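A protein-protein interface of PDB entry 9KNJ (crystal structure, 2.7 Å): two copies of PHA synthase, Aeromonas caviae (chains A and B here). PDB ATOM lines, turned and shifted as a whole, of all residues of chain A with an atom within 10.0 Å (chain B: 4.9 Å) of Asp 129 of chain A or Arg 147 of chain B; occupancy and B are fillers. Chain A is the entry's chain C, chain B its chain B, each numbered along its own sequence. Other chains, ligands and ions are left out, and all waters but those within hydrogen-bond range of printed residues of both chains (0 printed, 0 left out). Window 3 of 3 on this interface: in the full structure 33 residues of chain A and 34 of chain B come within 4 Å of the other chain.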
ATOM      1  N   PRO A  56       8.368 -12.729 -10.680  1.00  0.00           N
ATOM      2  CA  PRO A  56       9.485 -12.234 -11.478  1.00  0.00           C
ATOM      3  C   PRO A  56       9.166 -10.850 -12.057  1.00  0.00           C
ATOM      4  O   PRO A  56       8.016 -10.600 -12.331  1.00  0.00           O
ATOM      5  CB  PRO A  56       9.554 -13.236 -12.635  1.00  0.00           C
ATOM      6  CG  PRO A  56       8.744 -14.421 -12.172  1.00  0.00           C
ATOM      7  CD  PRO A  56       7.644 -13.810 -11.338  1.00  0.00           C
ATOM      8  N   TRP A  57      10.179 -10.003 -12.250  1.00  0.00           N
ATOM      9  CA  TRP A  57       9.893  -8.709 -12.856  1.00  0.00           C
ATOM     10  C   TRP A  57       9.427  -8.845 -14.300  1.00  0.00           C
ATOM     11  O   TRP A  57       8.785  -7.927 -14.820  1.00  0.00           O
ATOM     12  CB  TRP A  57      11.123  -7.801 -12.782  1.00  0.00           C
ATOM     13  CG  TRP A  57      12.254  -8.212 -13.679  1.00  0.00           C
ATOM     14  CD1 TRP A  57      13.305  -9.020 -13.355  1.00  0.00           C
ATOM     15  CD2 TRP A  57      12.452  -7.825 -15.048  1.00  0.00           C
ATOM     16  NE1 TRP A  57      14.143  -9.165 -14.437  1.00  0.00           N
ATOM     17  CE2 TRP A  57      13.641  -8.442 -15.487  1.00  0.00           C
ATOM     18  CE3 TRP A  57      11.738  -7.019 -15.943  1.00  0.00           C
ATOM     19  CZ2 TRP A  57      14.134  -8.279 -16.783  1.00  0.00           C
ATOM     20  CZ3 TRP A  57      12.228  -6.858 -17.229  1.00  0.00           C
ATOM     21  CH2 TRP A  57      13.415  -7.486 -17.635  1.00  0.00           C
ATOM     22  N   GLN A  58       9.733  -9.969 -14.954  1.00  0.00           N
ATOM     23  CA  GLN A  58       9.254 -10.191 -16.314  1.00  0.00           C
ATOM     24  C   GLN A  58       7.734 -10.310 -16.355  1.00  0.00           C
ATOM     25  O   GLN A  58       7.094  -9.866 -17.316  1.00  0.00           O
ATOM     26  CB  GLN A  58       9.911 -11.439 -16.901  1.00  0.00           C
ATOM     27  CG  GLN A  58      11.406 -11.289 -17.147  1.00  0.00           C
ATOM     28  CD  GLN A  58      12.245 -11.662 -15.933  1.00  0.00           C
ATOM     29  OE1 GLN A  58      11.724 -11.834 -14.829  1.00  0.00           O
ATOM     30  NE2 GLN A  58      13.553 -11.789 -16.136  1.00  0.00           N
ATOM     31  N   LEU A  59       7.141 -10.915 -15.324  1.00  0.00           N
ATOM     32  CA  LEU A  59       5.688 -11.041 -15.275  1.00  0.00           C
ATOM     33  C   LEU A  59       5.015  -9.676 -15.219  1.00  0.00           C
ATOM     34  O   LEU A  59       4.024  -9.436 -15.918  1.00  0.00           O
ATOM     35  CB  LEU A  59       5.277 -11.892 -14.072  1.00  0.00           C
ATOM     36  CG  LEU A  59       3.774 -12.027 -13.844  1.00  0.00           C
ATOM     37  CD1 LEU A  59       3.112 -12.789 -14.988  1.00  0.00           C
ATOM     38  CD2 LEU A  59       3.508 -12.704 -12.514  1.00  0.00           C
ATOM     39  N   ILE A  60       5.542  -8.766 -14.397  1.00  0.00           N
ATOM     40  CA  ILE A  60       4.973  -7.425 -14.311  1.00  0.00           C
ATOM     41  C   ILE A  60       5.225  -6.653 -15.601  1.00  0.00           C
ATOM     42  O   ILE A  60       4.384  -5.859 -16.039  1.00  0.00           O
ATOM     43  CB  ILE A  60       5.530  -6.684 -13.085  1.00  0.00           C
ATOM     44  CG1 ILE A  60       5.418  -7.564 -11.836  1.00  0.00           C
ATOM     45  CG2 ILE A  60       4.804  -5.357 -12.888  1.00  0.00           C
ATOM     46  CD1 ILE A  60       3.996  -7.890 -11.434  1.00  0.00           C
ATOM     47  N   ALA A  62       5.220  -7.904 -18.520  1.00  0.00           N
ATOM     48  CA  ALA A  62       4.209  -8.363 -19.467  1.00  0.00           C
ATOM     49  C   ALA A  62       2.896  -7.605 -19.289  1.00  0.00           C
ATOM     50  O   ALA A  62       2.228  -7.270 -20.274  1.00  0.00           O
ATOM     51  CB  ALA A  62       3.988  -9.866 -19.317  1.00  0.00           C
ATOM     52  N   LEU A 118      -4.470  -9.584 -30.611  1.00  0.00           N
ATOM     53  CA  LEU A 118      -3.048  -9.914 -30.684  1.00  0.00           C
ATOM     54  C   LEU A 118      -2.327  -9.503 -29.407  1.00  0.00           C
ATOM     55  O   LEU A 118      -1.408 -10.196 -28.951  1.00  0.00           O
ATOM     56  CB  LEU A 118      -2.395  -9.248 -31.898  1.00  0.00           C
ATOM     57  CG  LEU A 118      -2.481  -9.930 -33.271  1.00  0.00           C
ATOM     58  CD1 LEU A 118      -2.130 -11.411 -33.175  1.00  0.00           C
ATOM     59  CD2 LEU A 118      -3.823  -9.730 -33.943  1.00  0.00           C
ATOM     60  N   ALA A 121      -3.204 -12.055 -26.745  1.00  0.00           N
ATOM     61  CA  ALA A 121      -2.406 -13.255 -26.976  1.00  0.00           C
ATOM     62  C   ALA A 121      -0.951 -13.035 -26.583  1.00  0.00           C
ATOM     63  O   ALA A 121      -0.342 -13.890 -25.930  1.00  0.00           O
ATOM     64  CB  ALA A 121      -2.505 -13.683 -28.439  1.00  0.00           C
ATOM     65  N   ARG A 122      -0.379 -11.889 -26.958  1.00  0.00           N
ATOM     66  CA  ARG A 122       0.995 -11.598 -26.561  1.00  0.00           C
ATOM     67  C   ARG A 122       1.123 -11.565 -25.043  1.00  0.00           C
ATOM     68  O   ARG A 122       2.098 -12.081 -24.484  1.00  0.00           O
ATOM     69  CB  ARG A 122       1.456 -10.272 -27.174  1.00  0.00           C
ATOM     70  CG  ARG A 122       2.967 -10.078 -27.165  1.00  0.00           C
ATOM     71  CD  ARG A 122       3.538 -10.032 -28.575  1.00  0.00           C
ATOM     72  NE  ARG A 122       4.970  -9.749 -28.579  1.00  0.00           N
ATOM     73  CZ  ARG A 122       5.919 -10.675 -28.543  1.00  0.00           C
ATOM     74  NH1 ARG A 122       5.625 -11.964 -28.478  1.00  0.00           N
ATOM     75  NH2 ARG A 122       7.195 -10.299 -28.576  1.00  0.00           N
ATOM     76  N   HIS A 123       0.137 -10.975 -24.363  1.00  0.00           N
ATOM     77  CA  HIS A 123       0.151 -10.922 -22.905  1.00  0.00           C
ATOM     78  C   HIS A 123       0.077 -12.320 -22.298  1.00  0.00           C
ATOM     79  O   HIS A 123       0.773 -12.613 -21.319  1.00  0.00           O
ATOM     80  CB  HIS A 123      -1.004 -10.046 -22.415  1.00  0.00           C
ATOM     81  CG  HIS A 123      -1.277 -10.156 -20.948  1.00  0.00           C
ATOM     82  ND1 HIS A 123      -2.320 -10.901 -20.440  1.00  0.00           N
ATOM     83  CD2 HIS A 123      -0.657  -9.599 -19.881  1.00  0.00           C
ATOM     84  CE1 HIS A 123      -2.325 -10.807 -19.122  1.00  0.00           C
ATOM     85  NE2 HIS A 123      -1.327 -10.022 -18.757  1.00  0.00           N
ATOM     86  N   LEU A 124      -0.757 -13.198 -22.867  1.00  0.00           N
ATOM     87  CA  LEU A 124      -0.828 -14.576 -22.382  1.00  0.00           C
ATOM     88  C   LEU A 124       0.513 -15.283 -22.545  1.00  0.00           C
ATOM     89  O   LEU A 124       1.009 -15.925 -21.614  1.00  0.00           O
ATOM     90  CB  LEU A 124      -1.934 -15.341 -23.121  1.00  0.00           C
ATOM     91  CG  LEU A 124      -2.487 -16.679 -22.593  1.00  0.00           C
ATOM     92  CD1 LEU A 124      -3.734 -17.060 -23.377  1.00  0.00           C
ATOM     93  CD2 LEU A 124      -1.483 -17.830 -22.649  1.00  0.00           C
ATOM     94  N   LEU A 125       1.116 -15.177 -23.729  1.00  0.00           N
ATOM     95  CA  LEU A 125       2.371 -15.877 -23.977  1.00  0.00           C
ATOM     96  C   LEU A 125       3.492 -15.331 -23.098  1.00  0.00           C
ATOM     97  O   LEU A 125       4.314 -16.100 -22.588  1.00  0.00           O
ATOM     98  CB  LEU A 125       2.744 -15.781 -25.459  1.00  0.00           C
ATOM     99  CG  LEU A 125       2.127 -16.767 -26.465  1.00  0.00           C
ATOM    100  CD1 LEU A 125       2.683 -18.162 -26.256  1.00  0.00           C
ATOM    101  CD2 LEU A 125       0.607 -16.798 -26.412  1.00  0.00           C
ATOM    102  N   ALA A 126       3.537 -14.010 -22.907  1.00  0.00           N
ATOM    103  CA  ALA A 126       4.603 -13.408 -22.113  1.00  0.00           C
ATOM    104  C   ALA A 126       4.473 -13.754 -20.637  1.00  0.00           C
ATOM    105  O   ALA A 126       5.487 -13.861 -19.935  1.00  0.00           O
ATOM    106  CB  ALA A 126       4.608 -11.891 -22.296  1.00  0.00           C
ATOM    107  N   SER A 127       3.242 -13.908 -20.147  1.00  0.00           N
ATOM    108  CA  SER A 127       3.033 -14.255 -18.746  1.00  0.00           C
ATOM    109  C   SER A 127       3.458 -15.693 -18.466  1.00  0.00           C
ATOM    110  O   SER A 127       4.153 -15.964 -17.480  1.00  0.00           O
ATOM    111  CB  SER A 127       1.565 -14.041 -18.373  1.00  0.00           C
ATOM    112  OG  SER A 127       1.204 -12.673 -18.486  1.00  0.00           O
ATOM    113  N   VAL A 128       3.054 -16.629 -19.330  1.00  0.00           N
ATOM    114  CA  VAL A 128       3.418 -18.030 -19.143  1.00  0.00           C
ATOM    115  C   VAL A 128       4.930 -18.207 -19.223  1.00  0.00           C
ATOM    116  O   VAL A 128       5.518 -19.000 -18.478  1.00  0.00           O
ATOM    117  CB  VAL A 128       2.681 -18.916 -20.166  1.00  0.00           C
ATOM    118  CG1 VAL A 128       3.042 -20.381 -19.972  1.00  0.00           C
ATOM    119  CG2 VAL A 128       1.180 -18.726 -20.030  1.00  0.00           C
ATOM    120  N   ASP A 129       5.585 -17.466 -20.116  1.00  0.00           N
ATOM    121  CA  ASP A 129       7.034 -17.576 -20.232  1.00  0.00           C
ATOM    122  C   ASP A 129       7.749 -16.919 -19.058  1.00  0.00           C
ATOM    123  O   ASP A 129       8.847 -17.349 -18.686  1.00  0.00           O
ATOM    124  CB  ASP A 129       7.501 -16.973 -21.552  1.00  0.00           C
ATOM    125  CG  ASP A 129       7.231 -17.885 -22.727  1.00  0.00           C
ATOM    126  OD1 ASP A 129       7.216 -19.121 -22.525  1.00  0.00           O
ATOM    127  OD2 ASP A 129       7.030 -17.368 -23.847  1.00  0.00           O
ATOM    128  N   ALA A 130       7.152 -15.887 -18.460  1.00  0.00           N
ATOM    129  CA  ALA A 130       7.770 -15.255 -17.302  1.00  0.00           C
ATOM    130  C   ALA A 130       7.670 -16.121 -16.049  1.00  0.00           C
ATOM    131  O   ALA A 130       8.414 -15.889 -15.089  1.00  0.00           O
ATOM    132  CB  ALA A 130       7.139 -13.884 -17.047  1.00  0.00           C
ATOM    133  N   LEU A 131       6.781 -17.116 -16.046  1.00  0.00           N
ATOM    134  CA  LEU A 131       6.565 -17.988 -14.900  1.00  0.00           C
ATOM    135  C   LEU A 131       7.190 -19.366 -15.086  1.00  0.00           C
ATOM    136  O   LEU A 131       6.763 -20.324 -14.435  1.00  0.00           O
ATOM    137  CB  LEU A 131       5.068 -18.131 -14.623  1.00  0.00           C
ATOM    138  CG  LEU A 131       4.307 -16.869 -14.223  1.00  0.00           C
ATOM    139  CD1 LEU A 131       2.891 -17.231 -13.806  1.00  0.00           C
ATOM    140  CD2 LEU A 131       5.033 -16.128 -13.108  1.00  0.00           C
ATOM    141  N   GLU A 132       8.181 -19.490 -15.970  1.00  0.00           N
ATOM    142  CA  GLU A 132       8.760 -20.801 -16.246  1.00  0.00           C
ATOM    143  C   GLU A 132       9.614 -21.290 -15.080  1.00  0.00           C
ATOM    144  O   GLU A 132       9.525 -22.456 -14.678  1.00  0.00           O
ATOM    145  CB  GLU A 132       9.578 -20.751 -17.539  1.00  0.00           C
ATOM    146  CG  GLU A 132       8.864 -21.344 -18.751  1.00  0.00           C
ATOM    147  CD  GLU A 132       8.962 -22.857 -18.808  1.00  0.00           C
ATOM    148  OE1 GLU A 132      10.051 -23.369 -19.145  1.00  0.00           O
ATOM    149  OE2 GLU A 132       7.952 -23.533 -18.517  1.00  0.00           O
ATOM    150  N   GLY A 133      10.452 -20.410 -14.522  1.00  0.00           N
ATOM    151  CA  GLY A 133      11.301 -20.800 -13.408  1.00  0.00           C
ATOM    152  C   GLY A 133      10.621 -20.788 -12.056  1.00  0.00           C
ATOM    153  O   GLY A 133      11.154 -21.364 -11.103  1.00  0.00           O
ATOM    154  N   VAL A 134       9.466 -20.146 -11.952  1.00  0.00           N
ATOM    155  CA  VAL A 134       8.730 -20.088 -10.682  1.00  0.00           C
ATOM    156  C   VAL A 134       8.205 -21.480 -10.342  1.00  0.00           C
ATOM    157  O   VAL A 134       7.761 -22.208 -11.250  1.00  0.00           O
ATOM    158  CB  VAL A 134       7.596 -19.061 -10.781  1.00  0.00           C
ATOM    159  CG1 VAL A 134       6.440 -19.409  -9.861  1.00  0.00           C
ATOM    160  CG2 VAL A 134       8.122 -17.666 -10.466  1.00  0.00           C
ATOM    161  N   ARG A 139       3.249 -21.173  -8.585  1.00  0.00           N
ATOM    162  CA  ARG A 139       2.370 -20.804  -9.694  1.00  0.00           C
ATOM    163  C   ARG A 139       0.906 -21.062  -9.368  1.00  0.00           C
ATOM    164  O   ARG A 139       0.031 -20.320  -9.828  1.00  0.00           O
ATOM    165  CB  ARG A 139       2.763 -21.557 -10.965  1.00  0.00           C
ATOM    166  CG  ARG A 139       3.557 -20.721 -11.950  1.00  0.00           C
ATOM    167  CD  ARG A 139       3.932 -21.518 -13.188  1.00  0.00           C
ATOM    168  NE  ARG A 139       5.293 -22.035 -13.101  1.00  0.00           N
ATOM    169  CZ  ARG A 139       5.729 -23.122 -13.723  1.00  0.00           C
ATOM    170  NH1 ARG A 139       4.941 -23.822 -14.525  1.00  0.00           N
ATOM    171  NH2 ARG A 139       6.985 -23.517 -13.537  1.00  0.00           N
ATOM    172  N   ARG B 143       1.456 -23.733 -27.899  1.00  0.00           N
ATOM    173  CA  ARG B 143       2.157 -22.531 -27.466  1.00  0.00           C
ATOM    174  C   ARG B 143       3.184 -22.069 -28.490  1.00  0.00           C
ATOM    175  O   ARG B 143       3.528 -20.881 -28.512  1.00  0.00           O
ATOM    176  CB  ARG B 143       2.831 -22.767 -26.110  1.00  0.00           C
ATOM    177  CG  ARG B 143       2.880 -21.522 -25.236  1.00  0.00           C
ATOM    178  CD  ARG B 143       3.879 -21.631 -24.092  1.00  0.00           C
ATOM    179  NE  ARG B 143       4.970 -22.552 -24.378  1.00  0.00           N
ATOM    180  CZ  ARG B 143       5.358 -23.521 -23.560  1.00  0.00           C
ATOM    181  NH1 ARG B 143       4.762 -23.720 -22.396  1.00  0.00           N
ATOM    182  NH2 ARG B 143       6.367 -24.310 -23.920  1.00  0.00           N
ATOM    183  N   PHE B 144       3.674 -22.974 -29.341  1.00  0.00           N
ATOM    184  CA  PHE B 144       4.651 -22.590 -30.355  1.00  0.00           C
ATOM    185  C   PHE B 144       3.976 -21.957 -31.567  1.00  0.00           C
ATOM    186  O   PHE B 144       4.413 -20.908 -32.055  1.00  0.00           O
ATOM    187  CB  PHE B 144       5.476 -23.805 -30.776  1.00  0.00           C
ATOM    188  CG  PHE B 144       6.368 -23.550 -31.953  1.00  0.00           C
ATOM    189  CD1 PHE B 144       7.329 -22.554 -31.906  1.00  0.00           C
ATOM    190  CD2 PHE B 144       6.242 -24.301 -33.112  1.00  0.00           C
ATOM    191  CE1 PHE B 144       8.153 -22.312 -32.989  1.00  0.00           C
ATOM    192  CE2 PHE B 144       7.061 -24.065 -34.200  1.00  0.00           C
ATOM    193  CZ  PHE B 144       8.019 -23.069 -34.139  1.00  0.00           C
ATOM    194  N   PHE B 145       2.909 -22.582 -32.069  1.00  0.00           N
ATOM    195  CA  PHE B 145       2.239 -22.055 -33.252  1.00  0.00           C
ATOM    196  C   PHE B 145       1.478 -20.773 -32.941  1.00  0.00           C
ATOM    197  O   PHE B 145       1.277 -19.939 -33.833  1.00  0.00           O
ATOM    198  CB  PHE B 145       1.311 -23.116 -33.837  1.00  0.00           C
ATOM    199  CG  PHE B 145       2.023 -24.140 -34.678  1.00  0.00           C
ATOM    200  CD1 PHE B 145       2.787 -23.748 -35.768  1.00  0.00           C
ATOM    201  CD2 PHE B 145       1.946 -25.488 -34.367  1.00  0.00           C
ATOM    202  CE1 PHE B 145       3.449 -24.685 -36.544  1.00  0.00           C
ATOM    203  CE2 PHE B 145       2.607 -26.432 -35.134  1.00  0.00           C
ATOM    204  CZ  PHE B 145       3.360 -26.029 -36.225  1.00  0.00           C
ATOM    205  N   THR B 146       1.047 -20.598 -31.692  1.00  0.00           N
ATOM    206  CA  THR B 146       0.476 -19.318 -31.293  1.00  0.00           C
ATOM    207  C   THR B 146       1.524 -18.214 -31.351  1.00  0.00           C
ATOM    208  O   THR B 146       1.253 -17.118 -31.854  1.00  0.00           O
ATOM    209  CB  THR B 146      -0.125 -19.425 -29.893  1.00  0.00           C
ATOM    210  OG1 THR B 146      -1.177 -20.395 -29.905  1.00  0.00           O
ATOM    211  CG2 THR B 146      -0.691 -18.089 -29.450  1.00  0.00           C
ATOM    212  N   ARG B 147       2.734 -18.492 -30.860  1.00  0.00           N
ATOM    213  CA  ARG B 147       3.801 -17.498 -30.928  1.00  0.00           C
ATOM    214  C   ARG B 147       4.141 -17.162 -32.373  1.00  0.00           C
ATOM    215  O   ARG B 147       4.437 -16.006 -32.698  1.00  0.00           O
ATOM    216  CB  ARG B 147       5.039 -17.998 -30.182  1.00  0.00           C
ATOM    217  CG  ARG B 147       6.030 -16.899 -29.821  1.00  0.00           C
ATOM    218  CD  ARG B 147       6.749 -17.203 -28.517  1.00  0.00           C
ATOM    219  NE  ARG B 147       6.855 -18.637 -28.277  1.00  0.00           N
ATOM    220  CZ  ARG B 147       6.850 -19.197 -27.076  1.00  0.00           C
ATOM    221  NH1 ARG B 147       6.754 -18.471 -25.975  1.00  0.00           N
ATOM    222  NH2 ARG B 147       6.944 -20.521 -26.976  1.00  0.00           N
ATOM    223  N   GLN B 148       4.103 -18.164 -33.256  1.00  0.00           N
ATOM    224  CA  GLN B 148       4.359 -17.918 -34.672  1.00  0.00           C
ATOM    225  C   GLN B 148       3.304 -17.000 -35.275  1.00  0.00           C
ATOM    226  O   GLN B 148       3.628 -16.113 -36.073  1.00  0.00           O
ATOM    227  CB  GLN B 148       4.414 -19.242 -35.434  1.00  0.00           C
ATOM    228  CG  GLN B 148       5.298 -19.208 -36.670  1.00  0.00           C
ATOM    229  CD  GLN B 148       6.702 -19.707 -36.395  1.00  0.00           C
ATOM    230  OE1 GLN B 148       7.616 -18.920 -36.143  1.00  0.00           O
ATOM    231  NE2 GLN B 148       6.882 -21.023 -36.439  1.00  0.00           N
ATOM    232  N   TYR B 149       2.035 -17.197 -34.904  1.00  0.00           N
ATOM    233  CA  TYR B 149       0.960 -16.391 -35.475  1.00  0.00           C
ATOM    234  C   TYR B 149       1.059 -14.927 -35.051  1.00  0.00           C
ATOM    235  O   TYR B 149       0.875 -14.030 -35.880  1.00  0.00           O
ATOM    236  CB  TYR B 149      -0.400 -16.982 -35.089  1.00  0.00           C
ATOM    237  CG  TYR B 149      -1.598 -16.193 -35.587  1.00  0.00           C
ATOM    238  CD1 TYR B 149      -2.129 -16.426 -36.852  1.00  0.00           C
ATOM    239  CD2 TYR B 149      -2.187 -15.206 -34.803  1.00  0.00           C
ATOM    240  CE1 TYR B 149      -3.221 -15.703 -37.318  1.00  0.00           C
ATOM    241  CE2 TYR B 149      -3.278 -14.485 -35.259  1.00  0.00           C
ATOM    242  CZ  TYR B 149      -3.790 -14.736 -36.517  1.00  0.00           C
ATOM    243  OH  TYR B 149      -4.875 -14.014 -36.970  1.00  0.00           O
ATOM    244  N   VAL B 150       1.349 -14.659 -33.773  1.00  0.00           N
ATOM    245  CA  VAL B 150       1.365 -13.276 -33.291  1.00  0.00           C
ATOM    246  C   VAL B 150       2.446 -12.470 -33.997  1.00  0.00           C
ATOM    247  O   VAL B 150       2.227 -11.313 -34.377  1.00  0.00           O
ATOM    248  CB  VAL B 150       1.539 -13.228 -31.760  1.00  0.00           C
ATOM    249  CG1 VAL B 150       1.187 -11.843 -31.232  1.00  0.00           C
ATOM    250  CG2 VAL B 150       0.660 -14.263 -31.092  1.00  0.00           C
ATOM    251  N   ASN B 151       3.604 -13.086 -34.197  1.00  0.00           N
ATOM    252  CA  ASN B 151       4.719 -12.378 -34.873  1.00  0.00           C
ATOM    253  C   ASN B 151       4.352 -12.177 -36.344  1.00  0.00           C
ATOM    254  O   ASN B 151       4.595 -11.080 -36.868  1.00  0.00           O
ATOM    255  CB  ASN B 151       6.039 -13.123 -34.689  1.00  0.00           C
ATOM    256  CG  ASN B 151       6.466 -13.195 -33.239  1.00  0.00           C
ATOM    257  OD1 ASN B 151       6.657 -12.168 -32.592  1.00  0.00           O
ATOM    258  ND2 ASN B 151       6.611 -14.402 -32.716  1.00  0.00           N
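NH1 of Arg 147 of chain B lies within salt-bridge range of OD2 of Asp 129 of chain A (2.4 Å).
The backbone carbonyl oxygen (O) of Arg 147 of chain B is in hydrogen-bond range of the side-chain amide nitrogen (ND2) of Asn 151 of chain B, at 2.7 Å.
Tyr 149 of chain B touches Leu 118 of chain A.
Leu 118 of chain A touches Val 150 of chain B (O to CG1, 3.8 Å).
Val 150 of chain B touches Arg 122 of chain A (CG1 to CD, 3.98 Å).
CD1 of Leu 125 of chain A touches CG of Arg 143 of chain B, at 3.5 Å.
Thr 146 of chain B touches Leu 125 of chain A (CG2 to CD2, 3.5 Å).
Of the printed residues of chain A, Arg 147 of chain B touches Asp 129 (2.4 Å).
Thr 146 of chain B touches just one residue of chain A: Leu 125 (3.5 Å).
Of the printed residues of chain A, Val 150 of chain B touches Leu 118 (3.8 Å) and Arg 122 (3.98 Å).
Of the printed residues of chain A, Tyr 149 of chain B touches Leu 118 (3.9 Å).
Of the printed residues of chain A, Arg 143 of chain B touches Leu 125 (3.5 Å).
Of the printed residues of chain B, Leu 118 of chain A touches Tyr 149 and Val 150.
Gln 148 of chain B touches none of the printed residues of chain A.
The nearest residue of chain B that does not touch Asp 129 of chain A is Arg 143 of chain B (4.5 Å).
Hydrophobic or aromatic side chains of chain B that line the printed part of chain A: Tyr 149 and Val 150.
Of the 22 printed residues of chain A, 4 touch a printed residue of chain B.
Among the printed residues, 6 pairs touch across the chains.
Among the printed residues, Asp or Glu carboxylates within 4 Å of a Lys or Arg side-chain nitrogen of the other chain: Asp 129 of chain A with Arg 147 of chain B.
No position is printed for both chains.
Of the 6 pairs that touch across the chains among the printed residues, none has its exchanged pair printed and touching as well.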
